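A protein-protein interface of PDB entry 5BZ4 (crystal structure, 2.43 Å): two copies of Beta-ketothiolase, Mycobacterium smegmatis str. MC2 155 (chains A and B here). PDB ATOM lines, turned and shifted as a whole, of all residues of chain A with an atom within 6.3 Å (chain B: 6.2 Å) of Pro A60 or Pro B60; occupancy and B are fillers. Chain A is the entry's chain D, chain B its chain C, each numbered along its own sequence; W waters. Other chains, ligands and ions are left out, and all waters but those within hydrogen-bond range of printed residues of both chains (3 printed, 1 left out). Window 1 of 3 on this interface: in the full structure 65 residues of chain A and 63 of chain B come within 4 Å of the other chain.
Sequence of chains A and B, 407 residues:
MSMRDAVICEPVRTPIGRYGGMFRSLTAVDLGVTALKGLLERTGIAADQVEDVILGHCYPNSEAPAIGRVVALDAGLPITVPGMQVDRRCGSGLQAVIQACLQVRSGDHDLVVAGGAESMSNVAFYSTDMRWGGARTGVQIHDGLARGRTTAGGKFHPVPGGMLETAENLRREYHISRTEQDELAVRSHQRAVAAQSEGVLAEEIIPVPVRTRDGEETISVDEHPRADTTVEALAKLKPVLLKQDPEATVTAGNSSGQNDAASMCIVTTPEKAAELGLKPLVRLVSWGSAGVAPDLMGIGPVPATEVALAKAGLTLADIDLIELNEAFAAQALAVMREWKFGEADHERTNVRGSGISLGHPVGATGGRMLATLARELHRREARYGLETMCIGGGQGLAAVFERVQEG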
ATOM      1  N   HIS A  57       4.467  -3.580 -35.480  1.00  0.00           N
ATOM      2  CA  HIS A  57       3.988  -4.402 -34.382  1.00  0.00           C
ATOM      3  C   HIS A  57       2.582  -3.892 -34.154  1.00  0.00           C
ATOM      4  O   HIS A  57       2.405  -2.760 -33.697  1.00  0.00           O
ATOM      5  CB  HIS A  57       4.891  -4.216 -33.154  1.00  0.00           C
ATOM      6  CG  HIS A  57       4.597  -5.133 -32.006  1.00  0.00           C
ATOM      7  ND1 HIS A  57       4.274  -6.460 -32.159  1.00  0.00           N
ATOM      8  CD2 HIS A  57       4.590  -4.889 -30.671  1.00  0.00           C
ATOM      9  CE1 HIS A  57       4.074  -7.001 -30.967  1.00  0.00           C
ATOM     10  NE2 HIS A  57       4.263  -6.073 -30.052  1.00  0.00           N
ATOM     11  N   CYS A  58       1.585  -4.697 -34.506  1.00  0.00           N
ATOM     12  CA  CYS A  58       0.214  -4.202 -34.540  1.00  0.00           C
ATOM     13  C   CYS A  58      -0.598  -4.488 -33.287  1.00  0.00           C
ATOM     14  O   CYS A  58      -1.597  -3.819 -33.025  1.00  0.00           O
ATOM     15  CB  CYS A  58      -0.500  -4.773 -35.757  1.00  0.00           C
ATOM     16  SG  CYS A  58       0.233  -4.205 -37.289  1.00  0.00           S
ATOM     17  N   TYR A  59      -0.138  -5.453 -32.491  1.00  0.00           N
ATOM     18  CA  TYR A  59      -0.801  -5.793 -31.243  1.00  0.00           C
ATOM     19  C   TYR A  59       0.132  -5.621 -30.060  1.00  0.00           C
ATOM     20  O   TYR A  59       0.305  -6.535 -29.262  1.00  0.00           O
ATOM     21  CB  TYR A  59      -1.348  -7.217 -31.318  1.00  0.00           C
ATOM     22  CG  TYR A  59      -2.353  -7.354 -32.429  1.00  0.00           C
ATOM     23  CD1 TYR A  59      -3.672  -6.979 -32.241  1.00  0.00           C
ATOM     24  CD2 TYR A  59      -1.968  -7.808 -33.692  1.00  0.00           C
ATOM     25  CE1 TYR A  59      -4.594  -7.093 -33.266  1.00  0.00           C
ATOM     26  CE2 TYR A  59      -2.872  -7.907 -34.724  1.00  0.00           C
ATOM     27  CZ  TYR A  59      -4.182  -7.543 -34.508  1.00  0.00           C
ATOM     28  OH  TYR A  59      -5.092  -7.644 -35.522  1.00  0.00           O
ATOM     29  N   PRO A  60       0.727  -4.432 -29.923  1.00  0.00           N
ATOM     30  CA  PRO A  60       1.582  -4.233 -28.758  1.00  0.00           C
ATOM     31  C   PRO A  60       0.867  -4.385 -27.407  1.00  0.00           C
ATOM     32  O   PRO A  60      -0.335  -4.138 -27.290  1.00  0.00           O
ATOM     33  CB  PRO A  60       2.038  -2.792 -28.927  1.00  0.00           C
ATOM     34  CG  PRO A  60       0.928  -2.159 -29.657  1.00  0.00           C
ATOM     35  CD  PRO A  60       0.530  -3.168 -30.652  1.00  0.00           C
ATOM     36  N   ASN A  61       1.625  -4.773 -26.388  1.00  0.00           N
ATOM     37  CA  ASN A  61       1.165  -4.719 -25.010  1.00  0.00           C
ATOM     38  C   ASN A  61       2.394  -4.451 -24.130  1.00  0.00           C
ATOM     39  O   ASN A  61       3.518  -4.390 -24.646  1.00  0.00           O
ATOM     40  CB  ASN A  61       0.417  -6.008 -24.623  1.00  0.00           C
ATOM     41  CG  ASN A  61       1.319  -7.230 -24.568  1.00  0.00           C
ATOM     42  OD1 ASN A  61       2.463  -7.145 -24.152  1.00  0.00           O
ATOM     43  ND2 ASN A  61       0.792  -8.384 -24.984  1.00  0.00           N
ATOM     44  N   SER A  62       2.199  -4.311 -22.821  1.00  0.00           N
ATOM     45  CA  SER A  62       3.302  -3.921 -21.951  1.00  0.00           C
ATOM     46  C   SER A  62       4.317  -5.031 -21.672  1.00  0.00           C
ATOM     47  O   SER A  62       5.300  -4.782 -20.986  1.00  0.00           O
ATOM     48  CB  SER A  62       2.760  -3.381 -20.629  1.00  0.00           C
ATOM     49  OG  SER A  62       2.308  -2.052 -20.781  1.00  0.00           O
ATOM     50  N   ALA A  64       6.236  -5.815 -23.825  1.00  0.00           N
ATOM     51  CA  ALA A  64       7.345  -5.304 -24.636  1.00  0.00           C
ATOM     52  C   ALA A  64       7.047  -3.911 -25.159  1.00  0.00           C
ATOM     53  O   ALA A  64       6.715  -3.754 -26.333  1.00  0.00           O
ATOM     54  CB  ALA A  64       7.628  -6.247 -25.800  1.00  0.00           C
ATOM     55  N   GLN A  85       8.357   1.482 -31.846  1.00  0.00           N
ATOM     56  CA  GLN A  85       7.271   0.641 -32.321  1.00  0.00           C
ATOM     57  C   GLN A  85       6.364   1.479 -33.221  1.00  0.00           C
ATOM     58  O   GLN A  85       6.079   2.645 -32.897  1.00  0.00           O
ATOM     59  CB  GLN A  85       6.481   0.061 -31.130  1.00  0.00           C
ATOM     60  CG  GLN A  85       5.290  -0.795 -31.519  1.00  0.00           C
ATOM     61  CD  GLN A  85       3.961  -0.053 -31.490  1.00  0.00           C
ATOM     62  OE1 GLN A  85       3.722   0.809 -30.635  1.00  0.00           O
ATOM     63  NE2 GLN A  85       3.084  -0.392 -32.429  1.00  0.00           N
ATOM     64  N   ASP A  87       2.651   1.306 -35.778  1.00  0.00           N
ATOM     65  CA  ASP A  87       1.417   0.595 -36.090  1.00  0.00           C
ATOM     66  C   ASP A  87       0.576   1.310 -37.151  1.00  0.00           C
ATOM     67  O   ASP A  87      -0.130   2.272 -36.864  1.00  0.00           O
ATOM     68  CB  ASP A  87       0.593   0.405 -34.806  1.00  0.00           C
ATOM     69  CG  ASP A  87      -0.834  -0.044 -35.077  1.00  0.00           C
ATOM     70  OD1 ASP A  87      -1.091  -0.697 -36.103  1.00  0.00           O
ATOM     71  OD2 ASP A  87      -1.709   0.262 -34.246  1.00  0.00           O
ATOM     72  N   ARG A  89      -1.471  -0.884 -38.961  1.00  0.00           N
ATOM     73  CA  ARG A  89      -1.993  -2.240 -39.235  1.00  0.00           C
ATOM     74  C   ARG A  89      -1.114  -2.998 -40.242  1.00  0.00           C
ATOM     75  O   ARG A  89       0.108  -2.963 -40.134  1.00  0.00           O
ATOM     76  CB  ARG A  89      -3.444  -2.164 -39.730  1.00  0.00           C
ATOM     77  CG  ARG A  89      -4.368  -1.372 -38.801  1.00  0.00           C
ATOM     78  CD  ARG A  89      -4.818  -2.237 -37.661  1.00  0.00           C
ATOM     79  NE  ARG A  89      -3.911  -2.116 -36.538  1.00  0.00           N
ATOM     80  CZ  ARG A  89      -3.808  -3.011 -35.570  1.00  0.00           C
ATOM     81  NH1 ARG A  89      -4.578  -4.095 -35.582  1.00  0.00           N
ATOM     82  NH2 ARG A  89      -2.942  -2.811 -34.587  1.00  0.00           N
ATOM     83  N   GLU A 118       5.395 -10.081 -35.083  1.00  0.00           N
ATOM     84  CA  GLU A 118       4.048 -10.383 -34.617  1.00  0.00           C
ATOM     85  C   GLU A 118       3.928 -11.816 -34.137  1.00  0.00           C
ATOM     86  O   GLU A 118       4.281 -12.741 -34.869  1.00  0.00           O
ATOM     87  CB  GLU A 118       3.016 -10.119 -35.721  1.00  0.00           C
ATOM     88  CG  GLU A 118       1.646  -9.677 -35.205  1.00  0.00           C
ATOM     89  CD  GLU A 118       1.643  -8.239 -34.710  1.00  0.00           C
ATOM     90  OE1 GLU A 118       1.514  -8.021 -33.494  1.00  0.00           O
ATOM     91  OE2 GLU A 118       1.768  -7.328 -35.540  1.00  0.00           O
ATOM     92  N   HIS B  57       1.389   7.521 -28.749  1.00  0.00           N
ATOM     93  CA  HIS B  57       0.362   6.839 -27.999  1.00  0.00           C
ATOM     94  C   HIS B  57       0.997   5.582 -27.426  1.00  0.00           C
ATOM     95  O   HIS B  57       1.317   4.641 -28.179  1.00  0.00           O
ATOM     96  CB  HIS B  57      -0.807   6.529 -28.929  1.00  0.00           C
ATOM     97  CG  HIS B  57      -1.943   5.805 -28.280  1.00  0.00           C
ATOM     98  ND1 HIS B  57      -2.734   6.375 -27.314  1.00  0.00           N
ATOM     99  CD2 HIS B  57      -2.462   4.578 -28.523  1.00  0.00           C
ATOM    100  CE1 HIS B  57      -3.676   5.519 -26.960  1.00  0.00           C
ATOM    101  NE2 HIS B  57      -3.539   4.426 -27.679  1.00  0.00           N
ATOM    102  N   CYS B  58       1.190   5.570 -26.107  1.00  0.00           N
ATOM    103  CA  CYS B  58       2.024   4.564 -25.449  1.00  0.00           C
ATOM    104  C   CYS B  58       1.336   3.348 -24.827  1.00  0.00           C
ATOM    105  O   CYS B  58       2.011   2.365 -24.549  1.00  0.00           O
ATOM    106  CB  CYS B  58       2.858   5.251 -24.369  1.00  0.00           C
ATOM    107  SG  CYS B  58       3.986   6.466 -25.051  1.00  0.00           S
ATOM    108  N   TYR B  59       0.026   3.397 -24.591  1.00  0.00           N
ATOM    109  CA  TYR B  59      -0.682   2.181 -24.172  1.00  0.00           C
ATOM    110  C   TYR B  59      -1.819   1.849 -25.121  1.00  0.00           C
ATOM    111  O   TYR B  59      -2.984   1.839 -24.730  1.00  0.00           O
ATOM    112  CB  TYR B  59      -1.212   2.312 -22.738  1.00  0.00           C
ATOM    113  CG  TYR B  59      -0.133   2.680 -21.754  1.00  0.00           C
ATOM    114  CD1 TYR B  59       0.655   1.711 -21.151  1.00  0.00           C
ATOM    115  CD2 TYR B  59       0.117   3.998 -21.459  1.00  0.00           C
ATOM    116  CE1 TYR B  59       1.657   2.060 -20.272  1.00  0.00           C
ATOM    117  CE2 TYR B  59       1.096   4.349 -20.587  1.00  0.00           C
ATOM    118  CZ  TYR B  59       1.864   3.388 -19.999  1.00  0.00           C
ATOM    119  OH  TYR B  59       2.840   3.792 -19.127  1.00  0.00           O
ATOM    120  N   PRO B  60      -1.479   1.579 -26.384  1.00  0.00           N
ATOM    121  CA  PRO B  60      -2.529   1.222 -27.330  1.00  0.00           C
ATOM    122  C   PRO B  60      -3.214  -0.108 -26.981  1.00  0.00           C
ATOM    123  O   PRO B  60      -2.614  -0.995 -26.368  1.00  0.00           O
ATOM    124  CB  PRO B  60      -1.766   1.105 -28.652  1.00  0.00           C
ATOM    125  CG  PRO B  60      -0.400   0.687 -28.240  1.00  0.00           C
ATOM    126  CD  PRO B  60      -0.134   1.421 -26.974  1.00  0.00           C
ATOM    127  N   ASN B  61      -4.477  -0.220 -27.372  1.00  0.00           N
ATOM    128  CA  ASN B  61      -5.213  -1.468 -27.322  1.00  0.00           C
ATOM    129  C   ASN B  61      -6.167  -1.430 -28.507  1.00  0.00           C
ATOM    130  O   ASN B  61      -6.219  -0.421 -29.224  1.00  0.00           O
ATOM    131  CB  ASN B  61      -5.943  -1.643 -25.979  1.00  0.00           C
ATOM    132  CG  ASN B  61      -6.794  -0.450 -25.621  1.00  0.00           C
ATOM    133  OD1 ASN B  61      -7.482   0.119 -26.474  1.00  0.00           O
ATOM    134  ND2 ASN B  61      -6.753  -0.056 -24.353  1.00  0.00           N
ATOM    135  N   SER B  62      -6.915  -2.510 -28.712  1.00  0.00           N
ATOM    136  CA  SER B  62      -7.807  -2.638 -29.862  1.00  0.00           C
ATOM    137  C   SER B  62      -9.102  -1.841 -29.750  1.00  0.00           C
ATOM    138  O   SER B  62      -9.994  -2.010 -30.562  1.00  0.00           O
ATOM    139  CB  SER B  62      -8.126  -4.109 -30.080  1.00  0.00           C
ATOM    140  OG  SER B  62      -6.953  -4.834 -30.412  1.00  0.00           O
ATOM    141  N   ALA B  64      -8.778   1.219 -30.165  1.00  0.00           N
ATOM    142  CA  ALA B  64      -8.385   2.206 -31.170  1.00  0.00           C
ATOM    143  C   ALA B  64      -7.067   1.814 -31.810  1.00  0.00           C
ATOM    144  O   ALA B  64      -6.024   2.309 -31.413  1.00  0.00           O
ATOM    145  CB  ALA B  64      -8.283   3.588 -30.562  1.00  0.00           C
ATOM    146  N   GLN B  85       0.185   5.143 -35.537  1.00  0.00           N
ATOM    147  CA  GLN B  85       0.549   5.248 -34.131  1.00  0.00           C
ATOM    148  C   GLN B  85       2.023   4.880 -33.906  1.00  0.00           C
ATOM    149  O   GLN B  85       2.531   3.935 -34.510  1.00  0.00           O
ATOM    150  CB  GLN B  85      -0.391   4.359 -33.296  1.00  0.00           C
ATOM    151  CG  GLN B  85      -0.056   4.246 -31.811  1.00  0.00           C
ATOM    152  CD  GLN B  85       0.860   3.081 -31.523  1.00  0.00           C
ATOM    153  OE1 GLN B  85       0.672   1.980 -32.065  1.00  0.00           O
ATOM    154  NE2 GLN B  85       1.862   3.306 -30.674  1.00  0.00           N
ATOM    155  N   ASP B  87       5.327   4.477 -30.862  1.00  0.00           N
ATOM    156  CA  ASP B  87       5.673   4.340 -29.450  1.00  0.00           C
ATOM    157  C   ASP B  87       7.175   4.395 -29.265  1.00  0.00           C
ATOM    158  O   ASP B  87       7.890   3.489 -29.698  1.00  0.00           O
ATOM    159  CB  ASP B  87       5.119   3.026 -28.886  1.00  0.00           C
ATOM    160  CG  ASP B  87       5.580   2.738 -27.446  1.00  0.00           C
ATOM    161  OD1 ASP B  87       5.940   3.671 -26.713  1.00  0.00           O
ATOM    162  OD2 ASP B  87       5.556   1.558 -27.039  1.00  0.00           O
ATOM    163  N   ARG B  89       7.882   5.476 -25.879  1.00  0.00           N
ATOM    164  CA  ARG B  89       7.520   5.876 -24.517  1.00  0.00           C
ATOM    165  C   ARG B  89       7.357   7.376 -24.371  1.00  0.00           C
ATOM    166  O   ARG B  89       6.595   7.976 -25.114  1.00  0.00           O
ATOM    167  CB  ARG B  89       8.545   5.338 -23.508  1.00  0.00           C
ATOM    168  CG  ARG B  89       8.746   3.828 -23.579  1.00  0.00           C
ATOM    169  CD  ARG B  89       7.669   3.079 -22.827  1.00  0.00           C
ATOM    170  NE  ARG B  89       6.519   2.846 -23.689  1.00  0.00           N
ATOM    171  CZ  ARG B  89       5.285   2.585 -23.278  1.00  0.00           C
ATOM    172  NH1 ARG B  89       4.995   2.490 -21.991  1.00  0.00           N
ATOM    173  NH2 ARG B  89       4.334   2.407 -24.186  1.00  0.00           N
ATOM    174  N   GLU B 118      -3.103  10.416 -24.658  1.00  0.00           N
ATOM    175  CA  GLU B 118      -3.024   9.422 -23.613  1.00  0.00           C
ATOM    176  C   GLU B 118      -4.141   9.589 -22.565  1.00  0.00           C
ATOM    177  O   GLU B 118      -4.368  10.665 -22.019  1.00  0.00           O
ATOM    178  CB  GLU B 118      -1.635   9.460 -22.955  1.00  0.00           C
ATOM    179  CG  GLU B 118      -1.147   8.121 -22.391  1.00  0.00           C
ATOM    180  CD  GLU B 118      -0.567   7.216 -23.451  1.00  0.00           C
ATOM    181  OE1 GLU B 118      -1.207   6.201 -23.781  1.00  0.00           O
ATOM    182  OE2 GLU B 118       0.539   7.514 -23.937  1.00  0.00           O
HETATM  183  O   HOH W   1       3.266  -0.419 -22.715  1.00  0.00           O
HETATM  184  O   HOH W   2      -1.793   0.452 -31.797  1.00  0.00           O
HETATM  185  O   HOH W   3      -1.994  -3.308 -25.468  1.00  0.00           O
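The side-chain amide nitrogen (NE2) of Gln B85 sits at hydrogen-bond distance from the side-chain amide oxygen (OE1) of Gln A85 (3.1 Å).
The backbone NH (N) of Asp A87 is in hydrogen-bond range of the backbone carbonyl oxygen (O) of Gln B85.
The backbone NH (N) of Asp B87 is in hydrogen-bond range of the backbone carbonyl oxygen (O) of Gln A85 (2.8 Å).
Pro B60 touches its own counterpart, Pro A60.
Gln A85 touches its own counterpart, Gln B85.
Gln A85 touches Asp B87, and with the chains exchanged Asp A87 touches Gln B85.
11 positions are printed for both chains.
The backbone carbonyl oxygen of His B57 lies within hydrogen-bond range of the side-chain amide nitrogen of Gln B85, at 2.9 Å.
OD1 of Asp B87 sits at hydrogen-bond distance from SG of Cys B58, at 3.8 Å.
The side-chain carboxylate (OD1) of Asp B87 is in salt-bridge range of the guanidinium group (NE) of Arg B89, 3.2 Å away.
The backbone carbonyl oxygen (O) of His A57 is in hydrogen-bond range of the side-chain amide nitrogen (NE2) of Gln A85 (2.8 Å).
OD1 of Asp A87 lies within salt-bridge range of NE of Arg A89 (3.2 Å).
Among the printed residues, 4 pairs touch across the chains.
Water W2 lies within hydrogen-bond range of the side-chain carboxylate of Asp A87 and the side-chain amide oxygen of Gln B85.
Water W3 bridges the backbone carbonyl oxygen (O) of Pro B60 (2.6 Å) and the backbone carbonyl oxygen (O) of Pro A60 (2.6 Å).
Water W1 lies within hydrogen-bond range of the side-chain hydroxyl (OG) of Ser A62 and the guanidinium group (NH2) of Arg B89.
Pro A60 touches just one residue of chain B: Pro B60.
Ala A64 touches none of the printed residues of chain B.
Printed residues of chain B within 4 Å of Asp A87: Gln B85 (2.9 Å).
Cys B58 touches none of the printed residues of chain A.
Of chain A, only Pro A60 (3.4 Å) comes within 4 Å of Pro B60.
Of the printed residues of chain A, Gln B85 touches Gln A85 (3.1 Å) and Asp A87 (2.9 Å).
Of the printed residues of chain A, Asp B87 touches Gln A85.
The nearest residue of chain B that does not touch Pro A60 is Gln B85 (4.8 Å).
The nearest printed residue of chain B that does not touch Asp A87 is Ala B64 (5.6 Å).
Pro A60 touches Pro B60 (CG to CG, 3.4 Å).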
